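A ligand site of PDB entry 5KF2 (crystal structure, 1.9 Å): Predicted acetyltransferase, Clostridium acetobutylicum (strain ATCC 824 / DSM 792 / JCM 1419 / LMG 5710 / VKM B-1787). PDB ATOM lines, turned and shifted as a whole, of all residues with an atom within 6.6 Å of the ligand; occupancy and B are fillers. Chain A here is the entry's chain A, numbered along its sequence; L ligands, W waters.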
ATOM      1  N   PHE A 189      24.970  -1.352 -15.317  1.00  0.00           N
ATOM      2  CA  PHE A 189      23.561  -1.699 -15.337  1.00  0.00           C
ATOM      3  C   PHE A 189      22.934  -1.372 -16.675  1.00  0.00           C
ATOM      4  O   PHE A 189      21.962  -0.607 -16.735  1.00  0.00           O
ATOM      5  CB  PHE A 189      22.833  -0.957 -14.213  1.00  0.00           C
ATOM      6  CG  PHE A 189      23.319  -1.319 -12.828  1.00  0.00           C
ATOM      7  CD1 PHE A 189      23.097  -2.578 -12.302  1.00  0.00           C
ATOM      8  CD2 PHE A 189      24.010  -0.389 -12.056  1.00  0.00           C
ATOM      9  CE1 PHE A 189      23.546  -2.902 -11.026  1.00  0.00           C
ATOM     10  CE2 PHE A 189      24.456  -0.702 -10.787  1.00  0.00           C
ATOM     11  CZ  PHE A 189      24.221  -1.954 -10.271  1.00  0.00           C
ATOM     12  N   TRP A 193      17.647  -1.284 -16.682  1.00  0.00           N
ATOM     13  CA  TRP A 193      17.770  -0.075 -15.892  1.00  0.00           C
ATOM     14  C   TRP A 193      18.227   1.152 -16.690  1.00  0.00           C
ATOM     15  O   TRP A 193      17.625   2.247 -16.573  1.00  0.00           O
ATOM     16  CB  TRP A 193      18.642  -0.330 -14.643  1.00  0.00           C
ATOM     17  CG  TRP A 193      17.928  -1.168 -13.588  1.00  0.00           C
ATOM     18  CD1 TRP A 193      16.664  -1.746 -13.682  1.00  0.00           C
ATOM     19  CD2 TRP A 193      18.425  -1.526 -12.305  1.00  0.00           C
ATOM     20  NE1 TRP A 193      16.371  -2.408 -12.514  1.00  0.00           N
ATOM     21  CE2 TRP A 193      17.428  -2.299 -11.660  1.00  0.00           C
ATOM     22  CE3 TRP A 193      19.612  -1.253 -11.612  1.00  0.00           C
ATOM     23  CZ2 TRP A 193      17.589  -2.817 -10.362  1.00  0.00           C
ATOM     24  CZ3 TRP A 193      19.770  -1.781 -10.328  1.00  0.00           C
ATOM     25  CH2 TRP A 193      18.762  -2.542  -9.712  1.00  0.00           C
ATOM     26  N   PRO A 252      14.792   1.651  -8.564  1.00  0.00           N
ATOM     27  CA  PRO A 252      15.931   0.850  -8.130  1.00  0.00           C
ATOM     28  C   PRO A 252      17.073   1.590  -7.386  1.00  0.00           C
ATOM     29  O   PRO A 252      17.040   2.812  -7.161  1.00  0.00           O
ATOM     30  CB  PRO A 252      16.410   0.222  -9.419  1.00  0.00           C
ATOM     31  CG  PRO A 252      16.113   1.236 -10.472  1.00  0.00           C
ATOM     32  CD  PRO A 252      14.804   1.888 -10.018  1.00  0.00           C
ATOM     33  N   ILE A 253      18.014   0.786  -6.913  1.00  0.00           N
ATOM     34  CA  ILE A 253      19.222   1.264  -6.228  1.00  0.00           C
ATOM     35  C   ILE A 253      20.379   0.337  -6.655  1.00  0.00           C
ATOM     36  O   ILE A 253      20.216  -0.883  -6.809  1.00  0.00           O
ATOM     37  CB  ILE A 253      18.988   1.291  -4.722  1.00  0.00           C
ATOM     38  CG1 ILE A 253      20.209   1.832  -3.978  1.00  0.00           C
ATOM     39  CG2 ILE A 253      18.728  -0.136  -4.191  1.00  0.00           C
ATOM     40  CD1 ILE A 253      19.884   2.227  -2.554  1.00  0.00           C
ATOM     41  N   GLY A 254      21.566   0.908  -6.894  1.00  0.00           N
ATOM     42  CA  GLY A 254      22.691   0.138  -7.389  1.00  0.00           C
ATOM     43  C   GLY A 254      24.006   0.825  -7.147  1.00  0.00           C
ATOM     44  O   GLY A 254      24.070   2.054  -7.117  1.00  0.00           O
ATOM     45  N   ILE A 255      25.040   0.009  -7.009  1.00  0.00           N
ATOM     46  CA  ILE A 255      26.405   0.419  -6.729  1.00  0.00           C
ATOM     47  C   ILE A 255      27.301  -0.350  -7.696  1.00  0.00           C
ATOM     48  O   ILE A 255      27.142  -1.560  -7.888  1.00  0.00           O
ATOM     49  CB  ILE A 255      26.767   0.050  -5.277  1.00  0.00           C
ATOM     50  CG1 ILE A 255      26.026   0.978  -4.325  1.00  0.00           C
ATOM     51  CG2 ILE A 255      28.265   0.117  -4.996  1.00  0.00           C
ATOM     52  CD1 ILE A 255      26.588   2.382  -4.266  1.00  0.00           C
ATOM     53  N   ASP A 256      28.235   0.374  -8.308  1.00  0.00           N
ATOM     54  CA  ASP A 256      29.313  -0.211  -9.114  1.00  0.00           C
ATOM     55  C   ASP A 256      29.884  -1.447  -8.430  1.00  0.00           C
ATOM     56  O   ASP A 256      30.225  -1.387  -7.244  1.00  0.00           O
ATOM     57  CB  ASP A 256      30.414   0.839  -9.292  1.00  0.00           C
ATOM     58  CG  ASP A 256      31.483   0.427 -10.304  1.00  0.00           C
ATOM     59  OD1 ASP A 256      32.023  -0.703 -10.230  1.00  0.00           O
ATOM     60  OD2 ASP A 256      31.783   1.274 -11.185  1.00  0.00           O
ATOM     61  N   LYS A 257      29.995  -2.565  -9.149  1.00  0.00           N
ATOM     62  CA  LYS A 257      30.472  -3.844  -8.601  1.00  0.00           C
ATOM     63  C   LYS A 257      31.797  -3.789  -7.834  1.00  0.00           C
ATOM     64  O   LYS A 257      31.980  -4.474  -6.836  1.00  0.00           O
ATOM     65  CB  LYS A 257      30.682  -4.856  -9.718  1.00  0.00           C
ATOM     66  CG  LYS A 257      30.840  -6.294  -9.225  1.00  0.00           C
ATOM     67  CD  LYS A 257      31.849  -7.093 -10.041  1.00  0.00           C
ATOM     68  CE  LYS A 257      31.595  -7.036 -11.540  1.00  0.00           C
ATOM     69  NZ  LYS A 257      30.167  -7.269 -11.897  1.00  0.00           N
ATOM     70  N   TYR A 259      32.841  -1.580  -6.041  1.00  0.00           N
ATOM     71  CA  TYR A 259      32.620  -0.862  -4.783  1.00  0.00           C
ATOM     72  C   TYR A 259      31.637  -1.554  -3.825  1.00  0.00           C
ATOM     73  O   TYR A 259      31.218  -0.961  -2.828  1.00  0.00           O
ATOM     74  CB  TYR A 259      32.085   0.544  -5.087  1.00  0.00           C
ATOM     75  CG  TYR A 259      33.124   1.454  -5.692  1.00  0.00           C
ATOM     76  CD1 TYR A 259      33.841   2.334  -4.888  1.00  0.00           C
ATOM     77  CD2 TYR A 259      33.410   1.436  -7.055  1.00  0.00           C
ATOM     78  CE1 TYR A 259      34.807   3.172  -5.426  1.00  0.00           C
ATOM     79  CE2 TYR A 259      34.372   2.262  -7.597  1.00  0.00           C
ATOM     80  CZ  TYR A 259      35.070   3.129  -6.778  1.00  0.00           C
ATOM     81  OH  TYR A 259      36.034   3.989  -7.259  1.00  0.00           O
ATOM     82  N   ARG A 260      31.258  -2.798  -4.113  1.00  0.00           N
ATOM     83  CA  ARG A 260      30.191  -3.462  -3.334  1.00  0.00           C
ATOM     84  C   ARG A 260      30.686  -4.077  -2.022  1.00  0.00           C
ATOM     85  O   ARG A 260      31.886  -4.278  -1.823  1.00  0.00           O
ATOM     86  CB  ARG A 260      29.454  -4.504  -4.171  1.00  0.00           C
ATOM     87  CG  ARG A 260      28.347  -3.890  -5.012  1.00  0.00           C
ATOM     88  CD  ARG A 260      27.690  -4.883  -5.953  1.00  0.00           C
ATOM     89  NE  ARG A 260      27.139  -4.250  -7.152  1.00  0.00           N
ATOM     90  CZ  ARG A 260      26.968  -4.864  -8.324  1.00  0.00           C
ATOM     91  NH1 ARG A 260      27.288  -6.140  -8.468  1.00  0.00           N
ATOM     92  NH2 ARG A 260      26.478  -4.220  -9.368  1.00  0.00           N
ATOM     93  N   LYS A 261      29.763  -4.376  -1.124  1.00  0.00           N
ATOM     94  CA  LYS A 261      30.116  -4.966   0.168  1.00  0.00           C
ATOM     95  C   LYS A 261      31.170  -4.195   0.993  1.00  0.00           C
ATOM     96  O   LYS A 261      31.932  -4.792   1.737  1.00  0.00           O
ATOM     97  CB  LYS A 261      30.508  -6.443  -0.040  1.00  0.00           C
ATOM     98  CG  LYS A 261      29.353  -7.326  -0.500  1.00  0.00           C
ATOM     99  CD  LYS A 261      28.175  -7.243   0.467  1.00  0.00           C
ATOM    100  CE  LYS A 261      27.684  -8.577   1.037  1.00  0.00           C
ATOM    101  NZ  LYS A 261      26.771  -9.276   0.090  1.00  0.00           N
ATOM    102  N   GLN A 262      31.178  -2.859   0.857  1.00  0.00           N
ATOM    103  CA  GLN A 262      32.002  -1.958   1.647  1.00  0.00           C
ATOM    104  C   GLN A 262      31.134  -1.016   2.443  1.00  0.00           C
ATOM    105  O   GLN A 262      31.652  -0.006   2.884  1.00  0.00           O
ATOM    106  CB  GLN A 262      32.831  -0.998   0.782  1.00  0.00           C
ATOM    107  CG  GLN A 262      33.950  -1.536  -0.101  1.00  0.00           C
ATOM    108  CD  GLN A 262      34.654  -0.416  -0.887  1.00  0.00           C
ATOM    109  OE1 GLN A 262      34.822   0.733  -0.419  1.00  0.00           O
ATOM    110  NE2 GLN A 262      35.068  -0.739  -2.106  1.00  0.00           N
ATOM    111  N   GLY A 263      29.830  -1.251   2.578  1.00  0.00           N
ATOM    112  CA  GLY A 263      28.973  -0.309   3.281  1.00  0.00           C
ATOM    113  C   GLY A 263      28.434   0.863   2.481  1.00  0.00           C
ATOM    114  O   GLY A 263      27.686   1.681   2.999  1.00  0.00           O
ATOM    115  N   LEU A 264      28.747   0.923   1.192  1.00  0.00           N
ATOM    116  CA  LEU A 264      28.321   2.078   0.421  1.00  0.00           C
ATOM    117  C   LEU A 264      26.841   2.032   0.023  1.00  0.00           C
ATOM    118  O   LEU A 264      26.178   3.051  -0.031  1.00  0.00           O
ATOM    119  CB  LEU A 264      29.201   2.216  -0.804  1.00  0.00           C
ATOM    120  CG  LEU A 264      30.626   2.653  -0.396  1.00  0.00           C
ATOM    121  CD1 LEU A 264      31.627   2.526  -1.529  1.00  0.00           C
ATOM    122  CD2 LEU A 264      30.609   4.085   0.123  1.00  0.00           C
ATOM    123  N   GLY A 265      26.323   0.841  -0.256  1.00  0.00           N
ATOM    124  CA  GLY A 265      24.883   0.724  -0.595  1.00  0.00           C
ATOM    125  C   GLY A 265      24.065   1.134   0.600  1.00  0.00           C
ATOM    126  O   GLY A 265      23.100   1.896   0.509  1.00  0.00           O
ATOM    127  N   ARG A 266      24.470   0.661   1.772  1.00  0.00           N
ATOM    128  CA  ARG A 266      23.859   1.125   2.984  1.00  0.00           C
ATOM    129  C   ARG A 266      23.910   2.645   3.180  1.00  0.00           C
ATOM    130  O   ARG A 266      22.940   3.277   3.615  1.00  0.00           O
ATOM    131  CB  ARG A 266      24.479   0.349   4.164  1.00  0.00           C
ATOM    132  CG  ARG A 266      23.797   0.625   5.465  1.00  0.00           C
ATOM    133  CD  ARG A 266      24.606   0.103   6.639  1.00  0.00           C
ATOM    134  NE  ARG A 266      24.453  -1.343   6.793  1.00  0.00           N
ATOM    135  CZ  ARG A 266      25.368  -2.176   7.286  1.00  0.00           C
ATOM    136  NH1 ARG A 266      26.562  -1.736   7.669  1.00  0.00           N
ATOM    137  NH2 ARG A 266      25.084  -3.467   7.361  1.00  0.00           N
ATOM    138  N   LEU A 267      25.051   3.252   2.872  1.00  0.00           N
ATOM    139  CA  LEU A 267      25.122   4.694   2.989  1.00  0.00           C
ATOM    140  C   LEU A 267      24.144   5.344   2.005  1.00  0.00           C
ATOM    141  O   LEU A 267      23.409   6.270   2.355  1.00  0.00           O
ATOM    142  CB  LEU A 267      26.554   5.176   2.734  1.00  0.00           C
ATOM    143  CG  LEU A 267      26.722   6.698   2.809  1.00  0.00           C
ATOM    144  CD1 LEU A 267      26.387   7.232   4.195  1.00  0.00           C
ATOM    145  CD2 LEU A 267      28.139   7.040   2.362  1.00  0.00           C
ATOM    146  N   LEU A 268      24.183   4.873   0.758  1.00  0.00           N
ATOM    147  CA  LEU A 268      23.278   5.408  -0.267  1.00  0.00           C
ATOM    148  C   LEU A 268      21.808   5.294   0.159  1.00  0.00           C
ATOM    149  O   LEU A 268      21.005   6.231  -0.004  1.00  0.00           O
ATOM    150  CB  LEU A 268      23.538   4.749  -1.611  1.00  0.00           C
ATOM    151  CG  LEU A 268      22.548   5.060  -2.754  1.00  0.00           C
ATOM    152  CD1 LEU A 268      22.551   6.537  -3.094  1.00  0.00           C
ATOM    153  CD2 LEU A 268      22.880   4.274  -4.018  1.00  0.00           C
ATOM    154  N   GLU A 290      14.189  -9.272  -4.285  1.00  0.00           N
ATOM    155  CA  GLU A 290      14.396 -10.695  -4.085  1.00  0.00           C
ATOM    156  C   GLU A 290      14.526 -11.036  -2.610  1.00  0.00           C
ATOM    157  O   GLU A 290      14.933 -10.206  -1.771  1.00  0.00           O
ATOM    158  CB  GLU A 290      15.679 -11.101  -4.821  1.00  0.00           C
ATOM    159  CG  GLU A 290      15.487 -10.891  -6.306  1.00  0.00           C
ATOM    160  CD  GLU A 290      16.561 -11.551  -7.141  1.00  0.00           C
ATOM    161  OE1 GLU A 290      17.744 -11.477  -6.770  1.00  0.00           O
ATOM    162  OE2 GLU A 290      16.236 -12.126  -8.207  1.00  0.00           O
ATOM    163  N   ILE A 293      17.711 -10.178  -0.587  1.00  0.00           N
ATOM    164  CA  ILE A 293      18.043  -8.772  -0.315  1.00  0.00           C
ATOM    165  C   ILE A 293      17.128  -8.078   0.693  1.00  0.00           C
ATOM    166  O   ILE A 293      17.308  -6.902   1.054  1.00  0.00           O
ATOM    167  CB  ILE A 293      18.154  -7.956  -1.631  1.00  0.00           C
ATOM    168  CG1 ILE A 293      18.950  -6.648  -1.477  1.00  0.00           C
ATOM    169  CG2 ILE A 293      16.802  -7.594  -2.222  1.00  0.00           C
ATOM    170  CD1 ILE A 293      20.335  -6.855  -0.895  1.00  0.00           C
ATOM    171  N   PHE A 296      18.628  -6.170   3.831  1.00  0.00           N
ATOM    172  CA  PHE A 296      19.276  -4.886   3.453  1.00  0.00           C
ATOM    173  C   PHE A 296      18.333  -3.704   3.762  1.00  0.00           C
ATOM    174  O   PHE A 296      18.687  -2.737   4.464  1.00  0.00           O
ATOM    175  CB  PHE A 296      19.721  -4.951   1.982  1.00  0.00           C
ATOM    176  CG  PHE A 296      20.291  -3.648   1.423  1.00  0.00           C
ATOM    177  CD1 PHE A 296      21.436  -3.081   1.958  1.00  0.00           C
ATOM    178  CD2 PHE A 296      19.683  -3.000   0.346  1.00  0.00           C
ATOM    179  CE1 PHE A 296      21.967  -1.904   1.425  1.00  0.00           C
ATOM    180  CE2 PHE A 296      20.209  -1.837  -0.190  1.00  0.00           C
ATOM    181  CZ  PHE A 296      21.365  -1.279   0.364  1.00  0.00           C
ATOM    182  N   TYR A 297      17.089  -3.850   3.313  1.00  0.00           N
ATOM    183  CA  TYR A 297      16.101  -2.856   3.600  1.00  0.00           C
ATOM    184  C   TYR A 297      15.484  -2.985   4.982  1.00  0.00           C
ATOM    185  O   TYR A 297      14.996  -1.985   5.524  1.00  0.00           O
ATOM    186  CB  TYR A 297      14.982  -2.940   2.580  1.00  0.00           C
ATOM    187  CG  TYR A 297      15.491  -2.822   1.152  1.00  0.00           C
ATOM    188  CD1 TYR A 297      15.866  -1.578   0.629  1.00  0.00           C
ATOM    189  CD2 TYR A 297      15.637  -3.958   0.318  1.00  0.00           C
ATOM    190  CE1 TYR A 297      16.361  -1.471  -0.668  1.00  0.00           C
ATOM    191  CE2 TYR A 297      16.108  -3.836  -0.999  1.00  0.00           C
ATOM    192  CZ  TYR A 297      16.464  -2.576  -1.478  1.00  0.00           C
ATOM    193  OH  TYR A 297      16.903  -2.416  -2.779  1.00  0.00           O
HETATM  194  O1  LIG L   1      27.896  -3.331   1.672  1.00  0.00           O
HETATM  195  P1  LIG L   1      26.469  -2.887   1.738  1.00  0.00           P
HETATM  196  O2  LIG L   1      25.420  -3.474   2.631  1.00  0.00           O
HETATM  197  O3  LIG L   1      26.284  -1.300   1.800  1.00  0.00           O
HETATM  198  O4  LIG L   1      26.025  -3.460   0.305  1.00  0.00           O
HETATM  199  P2  LIG L   1      26.497  -3.112  -1.172  1.00  0.00           P
HETATM  200  O5  LIG L   1      26.793  -4.331  -2.010  1.00  0.00           O
HETATM  201  O6  LIG L   1      27.387  -1.918  -1.348  1.00  0.00           O
HETATM  202  O7  LIG L   1      25.066  -2.546  -1.678  1.00  0.00           O
HETATM  203  C1  LIG L   1      23.353  -3.175  -3.331  1.00  0.00           C
HETATM  204  C2  LIG L   1      23.971  -3.398  -1.967  1.00  0.00           C
HETATM  205  C3  LIG L   1      23.231  -1.759  -3.793  1.00  0.00           C
HETATM  206  C4  LIG L   1      21.986  -3.733  -3.555  1.00  0.00           C
HETATM  207  C5  LIG L   1      24.397  -3.718  -4.316  1.00  0.00           C
HETATM  208  O8  LIG L   1      24.852  -5.006  -3.949  1.00  0.00           O
HETATM  209  C6  LIG L   1      24.064  -3.773  -5.790  1.00  0.00           C
HETATM  210  O9  LIG L   1      24.068  -2.754  -6.454  1.00  0.00           O
HETATM  211  N1  LIG L   1      23.717  -4.906  -6.389  1.00  0.00           N
HETATM  212  C7  LIG L   1      23.131  -4.864  -7.732  1.00  0.00           C
HETATM  213  C8  LIG L   1      21.823  -4.051  -7.797  1.00  0.00           C
HETATM  214  C9  LIG L   1      20.660  -4.561  -6.949  1.00  0.00           C
HETATM  215  O10 LIG L   1      19.808  -3.750  -6.257  1.00  0.00           O
HETATM  216  N2  LIG L   1      20.575  -5.784  -6.948  1.00  0.00           N
HETATM  217  O   HOH W   1      29.724  -0.962  -0.517  1.00  0.00           O
HETATM  218  O   HOH W   2      16.911  -2.493  -7.065  1.00  0.00           O
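An oxygen (O3) of the ligand is in hydrogen-bond range of the backbone NH (N) of Arg 266 (2.7 Å). An oxygen (O3) of the ligand is in hydrogen-bond range of the backbone NH (N) of Gly 265 (3.0 Å). O1 of the ligand lies within hydrogen-bond range of N of Gly 263, 3.0 Å away. O9 of the ligand sits at hydrogen-bond distance from N of Ile 255 (3.0 Å). An oxygen (O5) of the ligand sits at hydrogen-bond distance from the backbone NH of Lys 261, 3.1 Å away. N of Leu 264 lies within hydrogen-bond range of O3 of the ligand (3.4 Å). An oxygen (O9) of the ligand lies close to the guanidinium group (NE) of Arg 260 (3.5 Å). The backbone NH (N) of Gln 262 lies within hydrogen-bond range of an oxygen (O1) of the ligand (3.4 Å).
The backbone carbonyl oxygen of Ile 255 sits at hydrogen-bond distance from the guanidinium group of Arg 260, at 2.8 Å.
The backbone carbonyl oxygen (O) of Ile 253 sits close to an oxygen (O10) of the ligand, at 2.9 Å. Phe 189 touches the ligand. Trp 193 touches the ligand (CH2 to O10, 3.8 Å). Gly 254 touches the ligand. CE1 of Phe 296 touches O2 of the ligand, 3.98 Å away. Hydrophobic or aromatic side chains within 4 Å of the ligand: Phe 189, Trp 193, Ile 255 and Phe 296. 13 residues have an atom within 4 Å of the ligand: Phe 189, Trp 193, Ile 253, Gly 254, Ile 255, Arg 260, Lys 261, Gln 262, Gly 263, Leu 264, Gly 265, Arg 266 and Phe 296. Along chain A the residues within 4 Å of the ligand span positions 189 to 296. The nearest printed residue that does not touch the ligand is Tyr 259 (4.2 Å).
Water W2 lies within hydrogen-bond range of O10 of the ligand and N of Ile 253.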
